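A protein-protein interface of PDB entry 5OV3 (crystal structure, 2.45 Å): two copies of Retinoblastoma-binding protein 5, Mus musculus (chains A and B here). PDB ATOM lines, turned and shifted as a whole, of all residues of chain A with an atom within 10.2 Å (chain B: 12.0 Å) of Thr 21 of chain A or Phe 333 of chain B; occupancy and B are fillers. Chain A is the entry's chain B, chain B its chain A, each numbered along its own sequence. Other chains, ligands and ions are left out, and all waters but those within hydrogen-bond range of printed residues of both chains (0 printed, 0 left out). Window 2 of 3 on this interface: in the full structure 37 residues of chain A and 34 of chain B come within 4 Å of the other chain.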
ATOM      1  N   ALA A  18      24.415   7.283  22.923  1.00  0.00           N
ATOM      2  CA  ALA A  18      23.852   7.819  21.689  1.00  0.00           C
ATOM      3  C   ALA A  18      24.080   6.881  20.497  1.00  0.00           C
ATOM      4  O   ALA A  18      24.816   5.892  20.586  1.00  0.00           O
ATOM      5  CB  ALA A  18      24.430   9.196  21.397  1.00  0.00           C
ATOM      6  N   ASP A  19      23.453   7.234  19.376  1.00  0.00           N
ATOM      7  CA  ASP A  19      23.280   6.336  18.243  1.00  0.00           C
ATOM      8  C   ASP A  19      24.603   6.103  17.511  1.00  0.00           C
ATOM      9  O   ASP A  19      25.651   6.663  17.848  1.00  0.00           O
ATOM     10  CB  ASP A  19      22.229   6.900  17.291  1.00  0.00           C
ATOM     11  CG  ASP A  19      22.461   8.370  16.975  1.00  0.00           C
ATOM     12  OD1 ASP A  19      23.204   9.031  17.735  1.00  0.00           O
ATOM     13  OD2 ASP A  19      21.894   8.867  15.974  1.00  0.00           O
ATOM     14  N   GLY A  20      24.540   5.261  16.479  1.00  0.00           N
ATOM     15  CA  GLY A  20      25.722   4.904  15.722  1.00  0.00           C
ATOM     16  C   GLY A  20      25.512   3.672  14.868  1.00  0.00           C
ATOM     17  O   GLY A  20      25.444   3.764  13.638  1.00  0.00           O
ATOM     18  N   THR A  21      25.392   2.509  15.514  1.00  0.00           N
ATOM     19  CA  THR A  21      25.281   1.252  14.786  1.00  0.00           C
ATOM     20  C   THR A  21      23.893   1.022  14.199  1.00  0.00           C
ATOM     21  O   THR A  21      23.757   0.194  13.288  1.00  0.00           O
ATOM     22  CB  THR A  21      25.639   0.075  15.695  1.00  0.00           C
ATOM     23  OG1 THR A  21      25.940  -1.063  14.888  1.00  0.00           O
ATOM     24  CG2 THR A  21      24.478  -0.268  16.603  1.00  0.00           C
ATOM     25  N   LEU A  22      22.862   1.717  14.696  1.00  0.00           N
ATOM     26  CA  LEU A  22      21.569   1.628  14.037  1.00  0.00           C
ATOM     27  C   LEU A  22      21.651   2.134  12.606  1.00  0.00           C
ATOM     28  O   LEU A  22      20.920   1.659  11.728  1.00  0.00           O
ATOM     29  CB  LEU A  22      20.524   2.414  14.822  1.00  0.00           C
ATOM     30  CG  LEU A  22      19.660   1.580  15.767  1.00  0.00           C
ATOM     31  CD1 LEU A  22      20.493   0.547  16.501  1.00  0.00           C
ATOM     32  CD2 LEU A  22      18.955   2.477  16.749  1.00  0.00           C
ATOM     33  N   ASP A  23      22.556   3.071  12.343  1.00  0.00           N
ATOM     34  CA  ASP A  23      22.635   3.661  11.017  1.00  0.00           C
ATOM     35  C   ASP A  23      22.997   2.622   9.963  1.00  0.00           C
ATOM     36  O   ASP A  23      22.387   2.585   8.888  1.00  0.00           O
ATOM     37  CB  ASP A  23      23.640   4.810  11.034  1.00  0.00           C
ATOM     38  CG  ASP A  23      23.241   5.909  12.014  1.00  0.00           C
ATOM     39  OD1 ASP A  23      22.310   6.686  11.702  1.00  0.00           O
ATOM     40  OD2 ASP A  23      23.842   5.979  13.112  1.00  0.00           O
ATOM     41  N   CYS A  24      23.951   1.738  10.265  1.00  0.00           N
ATOM     42  CA  CYS A  24      24.506   0.841   9.257  1.00  0.00           C
ATOM     43  C   CYS A  24      24.058  -0.618   9.364  1.00  0.00           C
ATOM     44  O   CYS A  24      24.419  -1.413   8.489  1.00  0.00           O
ATOM     45  CB  CYS A  24      26.040   0.893   9.297  1.00  0.00           C
ATOM     46  SG  CYS A  24      26.731   0.861  10.969  1.00  0.00           S
ATOM     47  N   ILE A  25      23.290  -1.005  10.390  1.00  0.00           N
ATOM     48  CA  ILE A  25      22.744  -2.361  10.421  1.00  0.00           C
ATOM     49  C   ILE A  25      21.647  -2.510   9.369  1.00  0.00           C
ATOM     50  O   ILE A  25      20.763  -1.652   9.226  1.00  0.00           O
ATOM     51  CB  ILE A  25      22.223  -2.705  11.823  1.00  0.00           C
ATOM     52  CG1 ILE A  25      23.405  -2.904  12.765  1.00  0.00           C
ATOM     53  CG2 ILE A  25      21.367  -3.972  11.789  1.00  0.00           C
ATOM     54  CD1 ILE A  25      23.015  -3.092  14.191  1.00  0.00           C
ATOM     55  N   SER A  26      21.704  -3.606   8.624  1.00  0.00           N
ATOM     56  CA  SER A  26      20.779  -3.853   7.532  1.00  0.00           C
ATOM     57  C   SER A  26      19.426  -4.353   8.033  1.00  0.00           C
ATOM     58  O   SER A  26      19.323  -5.058   9.039  1.00  0.00           O
ATOM     59  CB  SER A  26      21.363  -4.887   6.566  1.00  0.00           C
ATOM     60  OG  SER A  26      22.576  -4.443   6.008  1.00  0.00           O
ATOM     61  N   MET A  27      18.387  -4.003   7.296  1.00  0.00           N
ATOM     62  CA  MET A  27      17.074  -4.602   7.461  1.00  0.00           C
ATOM     63  C   MET A  27      16.860  -5.606   6.337  1.00  0.00           C
ATOM     64  O   MET A  27      17.039  -5.267   5.161  1.00  0.00           O
ATOM     65  CB  MET A  27      15.971  -3.537   7.425  1.00  0.00           C
ATOM     66  CG  MET A  27      16.177  -2.357   8.369  1.00  0.00           C
ATOM     67  SD  MET A  27      16.576  -2.872  10.048  1.00  0.00           S
ATOM     68  CE  MET A  27      14.932  -2.923  10.777  1.00  0.00           C
ATOM     69  N   ALA A  28      16.472  -6.828   6.699  1.00  0.00           N
ATOM     70  CA  ALA A  28      16.094  -7.819   5.701  1.00  0.00           C
ATOM     71  C   ALA A  28      14.710  -7.513   5.141  1.00  0.00           C
ATOM     72  O   ALA A  28      13.792  -7.157   5.881  1.00  0.00           O
ATOM     73  CB  ALA A  28      16.104  -9.211   6.321  1.00  0.00           C
ATOM     74  N   CYS A  44      18.458  -6.734   1.298  1.00  0.00           N
ATOM     75  CA  CYS A  44      18.341  -5.742   2.355  1.00  0.00           C
ATOM     76  C   CYS A  44      18.000  -4.347   1.835  1.00  0.00           C
ATOM     77  O   CYS A  44      17.956  -4.074   0.630  1.00  0.00           O
ATOM     78  CB  CYS A  44      19.630  -5.708   3.174  1.00  0.00           C
ATOM     79  SG  CYS A  44      19.963  -7.356   3.794  1.00  0.00           S
ATOM     80  N   ASN A  45      17.746  -3.461   2.795  1.00  0.00           N
ATOM     81  CA  ASN A  45      17.333  -2.101   2.470  1.00  0.00           C
ATOM     82  C   ASN A  45      18.478  -1.310   1.870  1.00  0.00           C
ATOM     83  O   ASN A  45      18.258  -0.442   1.017  1.00  0.00           O
ATOM     84  CB  ASN A  45      16.808  -1.408   3.717  1.00  0.00           C
ATOM     85  CG  ASN A  45      17.817  -1.387   4.850  1.00  0.00           C
ATOM     86  OD1 ASN A  45      18.646  -2.292   5.003  1.00  0.00           O
ATOM     87  ND2 ASN A  45      17.749  -0.351   5.661  1.00  0.00           N
ATOM     88  N   ASP A  46      19.700  -1.614   2.292  1.00  0.00           N
ATOM     89  CA  ASP A  46      20.897  -0.919   1.868  1.00  0.00           C
ATOM     90  C   ASP A  46      21.474  -1.484   0.579  1.00  0.00           C
ATOM     91  O   ASP A  46      22.640  -1.222   0.282  1.00  0.00           O
ATOM     92  CB  ASP A  46      21.938  -0.962   2.989  1.00  0.00           C
ATOM     93  CG  ASP A  46      22.278  -2.388   3.424  1.00  0.00           C
ATOM     94  OD1 ASP A  46      21.932  -3.341   2.682  1.00  0.00           O
ATOM     95  OD2 ASP A  46      22.899  -2.566   4.509  1.00  0.00           O
ATOM     96  N   GLY A  47      20.687  -2.263  -0.168  1.00  0.00           N
ATOM     97  CA  GLY A  47      21.114  -2.855  -1.427  1.00  0.00           C
ATOM     98  C   GLY A  47      21.975  -4.097  -1.325  1.00  0.00           C
ATOM     99  O   GLY A  47      22.311  -4.686  -2.361  1.00  0.00           O
ATOM    100  N   ARG A  48      22.351  -4.519  -0.128  1.00  0.00           N
ATOM    101  CA  ARG A  48      23.192  -5.690   0.010  1.00  0.00           C
ATOM    102  C   ARG A  48      22.364  -6.976  -0.080  1.00  0.00           C
ATOM    103  O   ARG A  48      21.155  -7.005   0.182  1.00  0.00           O
ATOM    104  CB  ARG A  48      23.963  -5.626   1.329  1.00  0.00           C
ATOM    105  CG  ARG A  48      25.263  -4.851   1.238  1.00  0.00           C
ATOM    106  CD  ARG A  48      25.556  -4.020   2.477  1.00  0.00           C
ATOM    107  NE  ARG A  48      25.089  -4.629   3.723  1.00  0.00           N
ATOM    108  CZ  ARG A  48      25.880  -4.999   4.733  1.00  0.00           C
ATOM    109  NH1 ARG A  48      25.359  -5.526   5.841  1.00  0.00           N
ATOM    110  NH2 ARG A  48      27.193  -4.839   4.639  1.00  0.00           N
ATOM    111  N   ILE A  49      23.033  -8.049  -0.479  1.00  0.00           N
ATOM    112  CA  ILE A  49      22.472  -9.391  -0.448  1.00  0.00           C
ATOM    113  C   ILE A  49      23.316 -10.208   0.525  1.00  0.00           C
ATOM    114  O   ILE A  49      24.525 -10.364   0.325  1.00  0.00           O
ATOM    115  CB  ILE A  49      22.452 -10.029  -1.845  1.00  0.00           C
ATOM    116  CG1 ILE A  49      21.657  -9.174  -2.822  1.00  0.00           C
ATOM    117  CG2 ILE A  49      21.870 -11.438  -1.812  1.00  0.00           C
ATOM    118  CD1 ILE A  49      21.599  -9.810  -4.200  1.00  0.00           C
ATOM    119  N   VAL A  50      22.691 -10.706   1.582  1.00  0.00           N
ATOM    120  CA  VAL A  50      23.368 -11.474   2.621  1.00  0.00           C
ATOM    121  C   VAL A  50      23.096 -12.954   2.405  1.00  0.00           C
ATOM    122  O   VAL A  50      21.939 -13.377   2.383  1.00  0.00           O
ATOM    123  CB  VAL A  50      22.891 -11.046   4.007  1.00  0.00           C
ATOM    124  CG1 VAL A  50      23.665 -11.761   5.060  1.00  0.00           C
ATOM    125  CG2 VAL A  50      23.040  -9.558   4.133  1.00  0.00           C
ATOM    126  N   ILE A  59      26.851 -16.123   8.626  1.00  0.00           N
ATOM    127  CA  ILE A  59      26.892 -15.502   7.308  1.00  0.00           C
ATOM    128  C   ILE A  59      28.081 -16.028   6.524  1.00  0.00           C
ATOM    129  O   ILE A  59      29.219 -16.009   7.008  1.00  0.00           O
ATOM    130  CB  ILE A  59      26.932 -13.973   7.434  1.00  0.00           C
ATOM    131  CG1 ILE A  59      25.553 -13.467   7.850  1.00  0.00           C
ATOM    132  CG2 ILE A  59      27.364 -13.328   6.122  1.00  0.00           C
ATOM    133  CD1 ILE A  59      25.633 -12.275   8.696  1.00  0.00           C
ATOM    134  N   ILE A  62      28.491 -11.593   1.758  1.00  0.00           N
ATOM    135  CA  ILE A  62      27.666 -10.406   1.591  1.00  0.00           C
ATOM    136  C   ILE A  62      27.967  -9.807   0.224  1.00  0.00           C
ATOM    137  O   ILE A  62      29.125  -9.528  -0.086  1.00  0.00           O
ATOM    138  CB  ILE A  62      27.931  -9.375   2.706  1.00  0.00           C
ATOM    139  CG1 ILE A  62      27.663  -9.996   4.078  1.00  0.00           C
ATOM    140  CG2 ILE A  62      27.097  -8.122   2.490  1.00  0.00           C
ATOM    141  CD1 ILE A  62      27.606  -8.983   5.191  1.00  0.00           C
ATOM    142  N   SER A  64      27.472  -6.621  -2.248  1.00  0.00           N
ATOM    143  CA  SER A  64      27.114  -5.202  -2.294  1.00  0.00           C
ATOM    144  C   SER A  64      26.543  -4.928  -3.675  1.00  0.00           C
ATOM    145  O   SER A  64      27.260  -4.619  -4.619  1.00  0.00           O
ATOM    146  CB  SER A  64      28.309  -4.322  -1.973  1.00  0.00           C
ATOM    147  OG  SER A  64      28.687  -4.500  -0.619  1.00  0.00           O
ATOM    148  N   GLY A 317      12.483  -6.331   9.252  1.00  0.00           N
ATOM    149  CA  GLY A 317      13.894  -6.453   8.940  1.00  0.00           C
ATOM    150  C   GLY A 317      14.648  -7.577   9.630  1.00  0.00           C
ATOM    151  O   GLY A 317      15.848  -7.726   9.373  1.00  0.00           O
ATOM    152  N   GLN B 326      32.710 -16.824   8.687  1.00  0.00           N
ATOM    153  CA  GLN B 326      33.602 -15.899   8.006  1.00  0.00           C
ATOM    154  C   GLN B 326      33.656 -14.568   8.753  1.00  0.00           C
ATOM    155  O   GLN B 326      32.881 -14.312   9.680  1.00  0.00           O
ATOM    156  CB  GLN B 326      33.188 -15.707   6.543  1.00  0.00           C
ATOM    157  CG  GLN B 326      33.535 -16.878   5.619  1.00  0.00           C
ATOM    158  CD  GLN B 326      33.124 -18.207   6.207  1.00  0.00           C
ATOM    159  OE1 GLN B 326      32.046 -18.317   6.797  1.00  0.00           O
ATOM    160  NE2 GLN B 326      33.992 -19.214   6.094  1.00  0.00           N
ATOM    161  N   VAL B 327      34.594 -13.718   8.318  1.00  0.00           N
ATOM    162  CA  VAL B 327      35.048 -12.512   9.014  1.00  0.00           C
ATOM    163  C   VAL B 327      33.894 -11.706   9.605  1.00  0.00           C
ATOM    164  O   VAL B 327      34.043 -11.053  10.645  1.00  0.00           O
ATOM    165  CB  VAL B 327      35.895 -11.639   8.062  1.00  0.00           C
ATOM    166  CG1 VAL B 327      35.118 -11.317   6.785  1.00  0.00           C
ATOM    167  CG2 VAL B 327      36.357 -10.361   8.752  1.00  0.00           C
ATOM    168  N   GLU B 328      32.731 -11.775   8.960  1.00  0.00           N
ATOM    169  CA  GLU B 328      31.590 -10.939   9.307  1.00  0.00           C
ATOM    170  C   GLU B 328      30.910 -11.373  10.601  1.00  0.00           C
ATOM    171  O   GLU B 328      31.521 -11.407  11.675  1.00  0.00           O
ATOM    172  CB  GLU B 328      30.554 -10.956   8.173  1.00  0.00           C
ATOM    173  CG  GLU B 328      31.116 -11.003   6.754  1.00  0.00           C
ATOM    174  CD  GLU B 328      31.472 -12.409   6.321  1.00  0.00           C
ATOM    175  OE1 GLU B 328      31.809 -12.612   5.134  1.00  0.00           O
ATOM    176  OE2 GLU B 328      31.407 -13.313   7.178  1.00  0.00           O
ATOM    177  N   ASN B 329      29.615 -11.665  10.480  1.00  0.00           N
ATOM    178  CA  ASN B 329      28.722 -12.133  11.533  1.00  0.00           C
ATOM    179  C   ASN B 329      28.420 -11.091  12.606  1.00  0.00           C
ATOM    180  O   ASN B 329      27.472 -11.274  13.379  1.00  0.00           O
ATOM    181  CB  ASN B 329      29.252 -13.423  12.144  1.00  0.00           C
ATOM    182  CG  ASN B 329      28.555 -14.637  11.566  1.00  0.00           C
ATOM    183  OD1 ASN B 329      29.176 -15.484  10.929  1.00  0.00           O
ATOM    184  ND2 ASN B 329      27.237 -14.696  11.743  1.00  0.00           N
ATOM    185  N   TRP B 330      29.204 -10.009  12.662  1.00  0.00           N
ATOM    186  CA  TRP B 330      28.713  -8.731  13.175  1.00  0.00           C
ATOM    187  C   TRP B 330      29.722  -7.614  12.954  1.00  0.00           C
ATOM    188  O   TRP B 330      29.378  -6.432  13.065  1.00  0.00           O
ATOM    189  CB  TRP B 330      28.346  -8.786  14.656  1.00  0.00           C
ATOM    190  CG  TRP B 330      27.365  -7.709  14.974  1.00  0.00           C
ATOM    191  CD1 TRP B 330      27.613  -6.528  15.608  1.00  0.00           C
ATOM    192  CD2 TRP B 330      25.980  -7.686  14.607  1.00  0.00           C
ATOM    193  NE1 TRP B 330      26.461  -5.783  15.686  1.00  0.00           N
ATOM    194  CE2 TRP B 330      25.445  -6.474  15.077  1.00  0.00           C
ATOM    195  CE3 TRP B 330      25.138  -8.581  13.939  1.00  0.00           C
ATOM    196  CZ2 TRP B 330      24.110  -6.139  14.909  1.00  0.00           C
ATOM    197  CZ3 TRP B 330      23.814  -8.241  13.769  1.00  0.00           C
ATOM    198  CH2 TRP B 330      23.314  -7.031  14.248  1.00  0.00           C
ATOM    199  N   SER B 331      30.964  -7.969  12.635  1.00  0.00           N
ATOM    200  CA  SER B 331      31.869  -6.953  12.117  1.00  0.00           C
ATOM    201  C   SER B 331      31.373  -6.349  10.803  1.00  0.00           C
ATOM    202  O   SER B 331      32.007  -5.417  10.291  1.00  0.00           O
ATOM    203  CB  SER B 331      33.268  -7.543  11.935  1.00  0.00           C
ATOM    204  OG  SER B 331      34.106  -6.641  11.235  1.00  0.00           O
ATOM    205  N   ALA B 332      30.251  -6.843  10.265  1.00  0.00           N
ATOM    206  CA  ALA B 332      29.733  -6.423   8.977  1.00  0.00           C
ATOM    207  C   ALA B 332      28.375  -5.742   9.047  1.00  0.00           C
ATOM    208  O   ALA B 332      27.826  -5.392   7.992  1.00  0.00           O
ATOM    209  CB  ALA B 332      29.626  -7.621   8.033  1.00  0.00           C
ATOM    210  N   PHE B 333      27.809  -5.552  10.240  1.00  0.00           N
ATOM    211  CA  PHE B 333      26.513  -4.894  10.405  1.00  0.00           C
ATOM    212  C   PHE B 333      25.459  -5.538   9.508  1.00  0.00           C
ATOM    213  O   PHE B 333      24.862  -4.907   8.640  1.00  0.00           O
ATOM    214  CB  PHE B 333      26.630  -3.394  10.122  1.00  0.00           C
ATOM    215  CG  PHE B 333      27.736  -2.722  10.865  1.00  0.00           C
ATOM    216  CD1 PHE B 333      27.626  -2.455  12.213  1.00  0.00           C
ATOM    217  CD2 PHE B 333      28.890  -2.344  10.215  1.00  0.00           C
ATOM    218  CE1 PHE B 333      28.646  -1.824  12.890  1.00  0.00           C
ATOM    219  CE2 PHE B 333      29.907  -1.716  10.896  1.00  0.00           C
ATOM    220  CZ  PHE B 333      29.785  -1.457  12.231  1.00  0.00           C
ATOM    221  N   ALA B 334      25.270  -6.821   9.703  1.00  0.00           N
ATOM    222  CA  ALA B 334      24.327  -7.591   8.916  1.00  0.00           C
ATOM    223  C   ALA B 334      22.975  -7.631   9.610  1.00  0.00           C
ATOM    224  O   ALA B 334      22.862  -7.317  10.800  1.00  0.00           O
ATOM    225  CB  ALA B 334      24.864  -8.998   8.704  1.00  0.00           C
ATOM    226  N   PRO B 335      21.909  -8.007   8.888  1.00  0.00           N
ATOM    227  CA  PRO B 335      20.591  -8.088   9.525  1.00  0.00           C
ATOM    228  C   PRO B 335      20.576  -9.165  10.590  1.00  0.00           C
ATOM    229  O   PRO B 335      21.344 -10.121  10.543  1.00  0.00           O
ATOM    230  CB  PRO B 335      19.650  -8.432   8.365  1.00  0.00           C
ATOM    231  CG  PRO B 335      20.501  -9.012   7.325  1.00  0.00           C
ATOM    232  CD  PRO B 335      21.836  -8.327   7.451  1.00  0.00           C
ATOM    233  N   ASP B 336      19.681  -9.010  11.550  1.00  0.00           N
ATOM    234  CA  ASP B 336      19.597  -9.959  12.642  1.00  0.00           C
ATOM    235  C   ASP B 336      18.880 -11.223  12.203  1.00  0.00           C
ATOM    236  O   ASP B 336      17.904 -11.174  11.450  1.00  0.00           O
ATOM    237  CB  ASP B 336      18.893  -9.335  13.846  1.00  0.00           C
ATOM    238  CG  ASP B 336      19.804  -8.396  14.619  1.00  0.00           C
ATOM    239  OD1 ASP B 336      19.816  -8.433  15.870  1.00  0.00           O
ATOM    240  OD2 ASP B 336      20.532  -7.612  13.977  1.00  0.00           O
ATOM    241  N   PHE B 337      19.375 -12.355  12.693  1.00  0.00           N
ATOM    242  CA  PHE B 337      18.845 -13.685  12.427  1.00  0.00           C
ATOM    243  C   PHE B 337      18.468 -14.301  13.761  1.00  0.00           C
ATOM    244  O   PHE B 337      19.295 -14.370  14.672  1.00  0.00           O
ATOM    245  CB  PHE B 337      19.878 -14.576  11.720  1.00  0.00           C
ATOM    246  CG  PHE B 337      20.092 -14.226  10.281  1.00  0.00           C
ATOM    247  CD1 PHE B 337      20.918 -13.159   9.924  1.00  0.00           C
ATOM    248  CD2 PHE B 337      19.465 -14.959   9.271  1.00  0.00           C
ATOM    249  CE1 PHE B 337      21.110 -12.806   8.571  1.00  0.00           C
ATOM    250  CE2 PHE B 337      19.644 -14.627   7.924  1.00  0.00           C
ATOM    251  CZ  PHE B 337      20.473 -13.535   7.575  1.00  0.00           C
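The side-chain amide oxygen (OD1) of Asn 329 of chain B sits at hydrogen-bond distance from the backbone NH (N) of Ile 59 of chain A.
The guanidinium group (NH1) of Arg 48 of chain A sits at hydrogen-bond distance from the backbone carbonyl oxygen (O) of Ala 332 of chain B, at 3.3 Å.
O of Phe 333 of chain B sits at hydrogen-bond distance from N of Ser 26 of chain A, at 3.4 Å.
O of Phe 333 of chain B lies within hydrogen-bond range of NH1 of Arg 48 of chain A, at 2.9 Å.
The backbone carbonyl oxygen (O) of Ile 59 of chain A sits close to the side-chain carboxylate (OE2) of Glu 328 of chain B (3.5 Å).
Among the printed residues, merely in contact across the chains: Thr 21 of chain A with Phe 333 of chain B (3.4 Å), Cys 24 of chain A with Phe 333 of chain B (3.4 Å), Ile 25 of chain A with Trp 330 of chain B (3.3 Å), Ile 25 of chain A with Phe 333 of chain B (3.8 Å), Ile 25 of chain A with Ala 334 of chain B (3.8 Å), Ser 26 of chain A with Pro 335 of chain B (3.3 Å), Ala 28 of chain A with Pro 335 of chain B (3.9 Å), Cys 44 of chain A with Pro 335 of chain B (3.9 Å), Arg 48 of chain A with Ala 334 of chain B (3.8 Å), Val 50 of chain A with Pro 335 of chain B (3.7 Å), Ile 59 of chain A with Gln 326 of chain B (3.7 Å), Ile 59 of chain A with Ala 334 of chain B (3.4 Å), Ile 62 of chain A with Ala 332 of chain B (3.7 Å) and Gly 317 of chain A with Pro 335 of chain B (3.996 Å).
Of the 22 printed residues of chain A, 11 touch a printed residue of chain B.
Of the 12 printed residues of chain B, 8 touch a printed residue of chain A.
Printed residues of chain B that touch a printed residue of chain A: Gln 326, Glu 328, Asn 329, Trp 330, Ala 332, Phe 333, Ala 334 and Pro 335.
Among the printed residues, 19 pairs touch across the chains.
Among the printed residues, no Asp or Glu carboxylate lies within 4 Å of a Lys or Arg side-chain nitrogen of the other chain.
Of chain B, only Phe 333 comes within 4 Å of Thr 21 of chain A.
Of the printed residues of chain A, Phe 333 of chain B touches Thr 21 (3.4 Å), Cys 24 (3.4 Å), Ile 25 (3.8 Å), Ser 26 (3.4 Å) and Arg 48 (2.9 Å).
No residue of chain B comes within 4 Å of Asp 19 of chain A.
Gly 20 of chain A touches none of the printed residues of chain B.
Asp 23 of chain A touches none of the printed residues of chain B.
Ile 25 of chain A touches three residues of chain B.
Of chain A, only Ile 25 (3.3 Å) comes within 4 Å of Trp 330 of chain B.
Ala 332 of chain B touches two residues of chain A.
Of chain A, only Ile 25, Arg 48 and Ile 59 come within 4 Å of Ala 334 of chain B.
Printed residues of chain B within 4 Å of Ala 28 of chain A: Pro 335 (3.9 Å).
Of the printed residues of chain B, Cys 44 of chain A touches Pro 335 (3.9 Å).
Of the printed residues of chain B, Ile 62 of chain A touches Ala 332.
Of the printed residues of chain B, Arg 48 of chain A touches Ala 332, Phe 333 and Ala 334.
Asp 46 of chain A touches none of the printed residues of chain B.
Ile 49 of chain A touches none of the printed residues of chain B.
The nearest residue of chain A that does not touch Phe 333 of chain B is Asp 46 of chain A (5.1 Å).
The nearest printed residue of chain B that does not touch Val 50 of chain A is Phe 337 of chain B (4.4 Å).
No position is printed for both chains.
OG of Ser 26 of chain A lies within hydrogen-bond range of OD2 of Asp 46 of chain A.
The side-chain hydroxyl (OG) of Ser 26 of chain A sits at hydrogen-bond distance from the guanidinium group (NH1) of Arg 48 of chain A, 3.0 Å away.
The backbone NH (N) of Ala 28 of chain A lies within hydrogen-bond range of the backbone carbonyl oxygen (O) of Gly 317 of chain A (2.9 Å).
OD2 of Asp 46 of chain A lies within salt-bridge range of NE of Arg 48 of chain A, 3.1 Å away.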
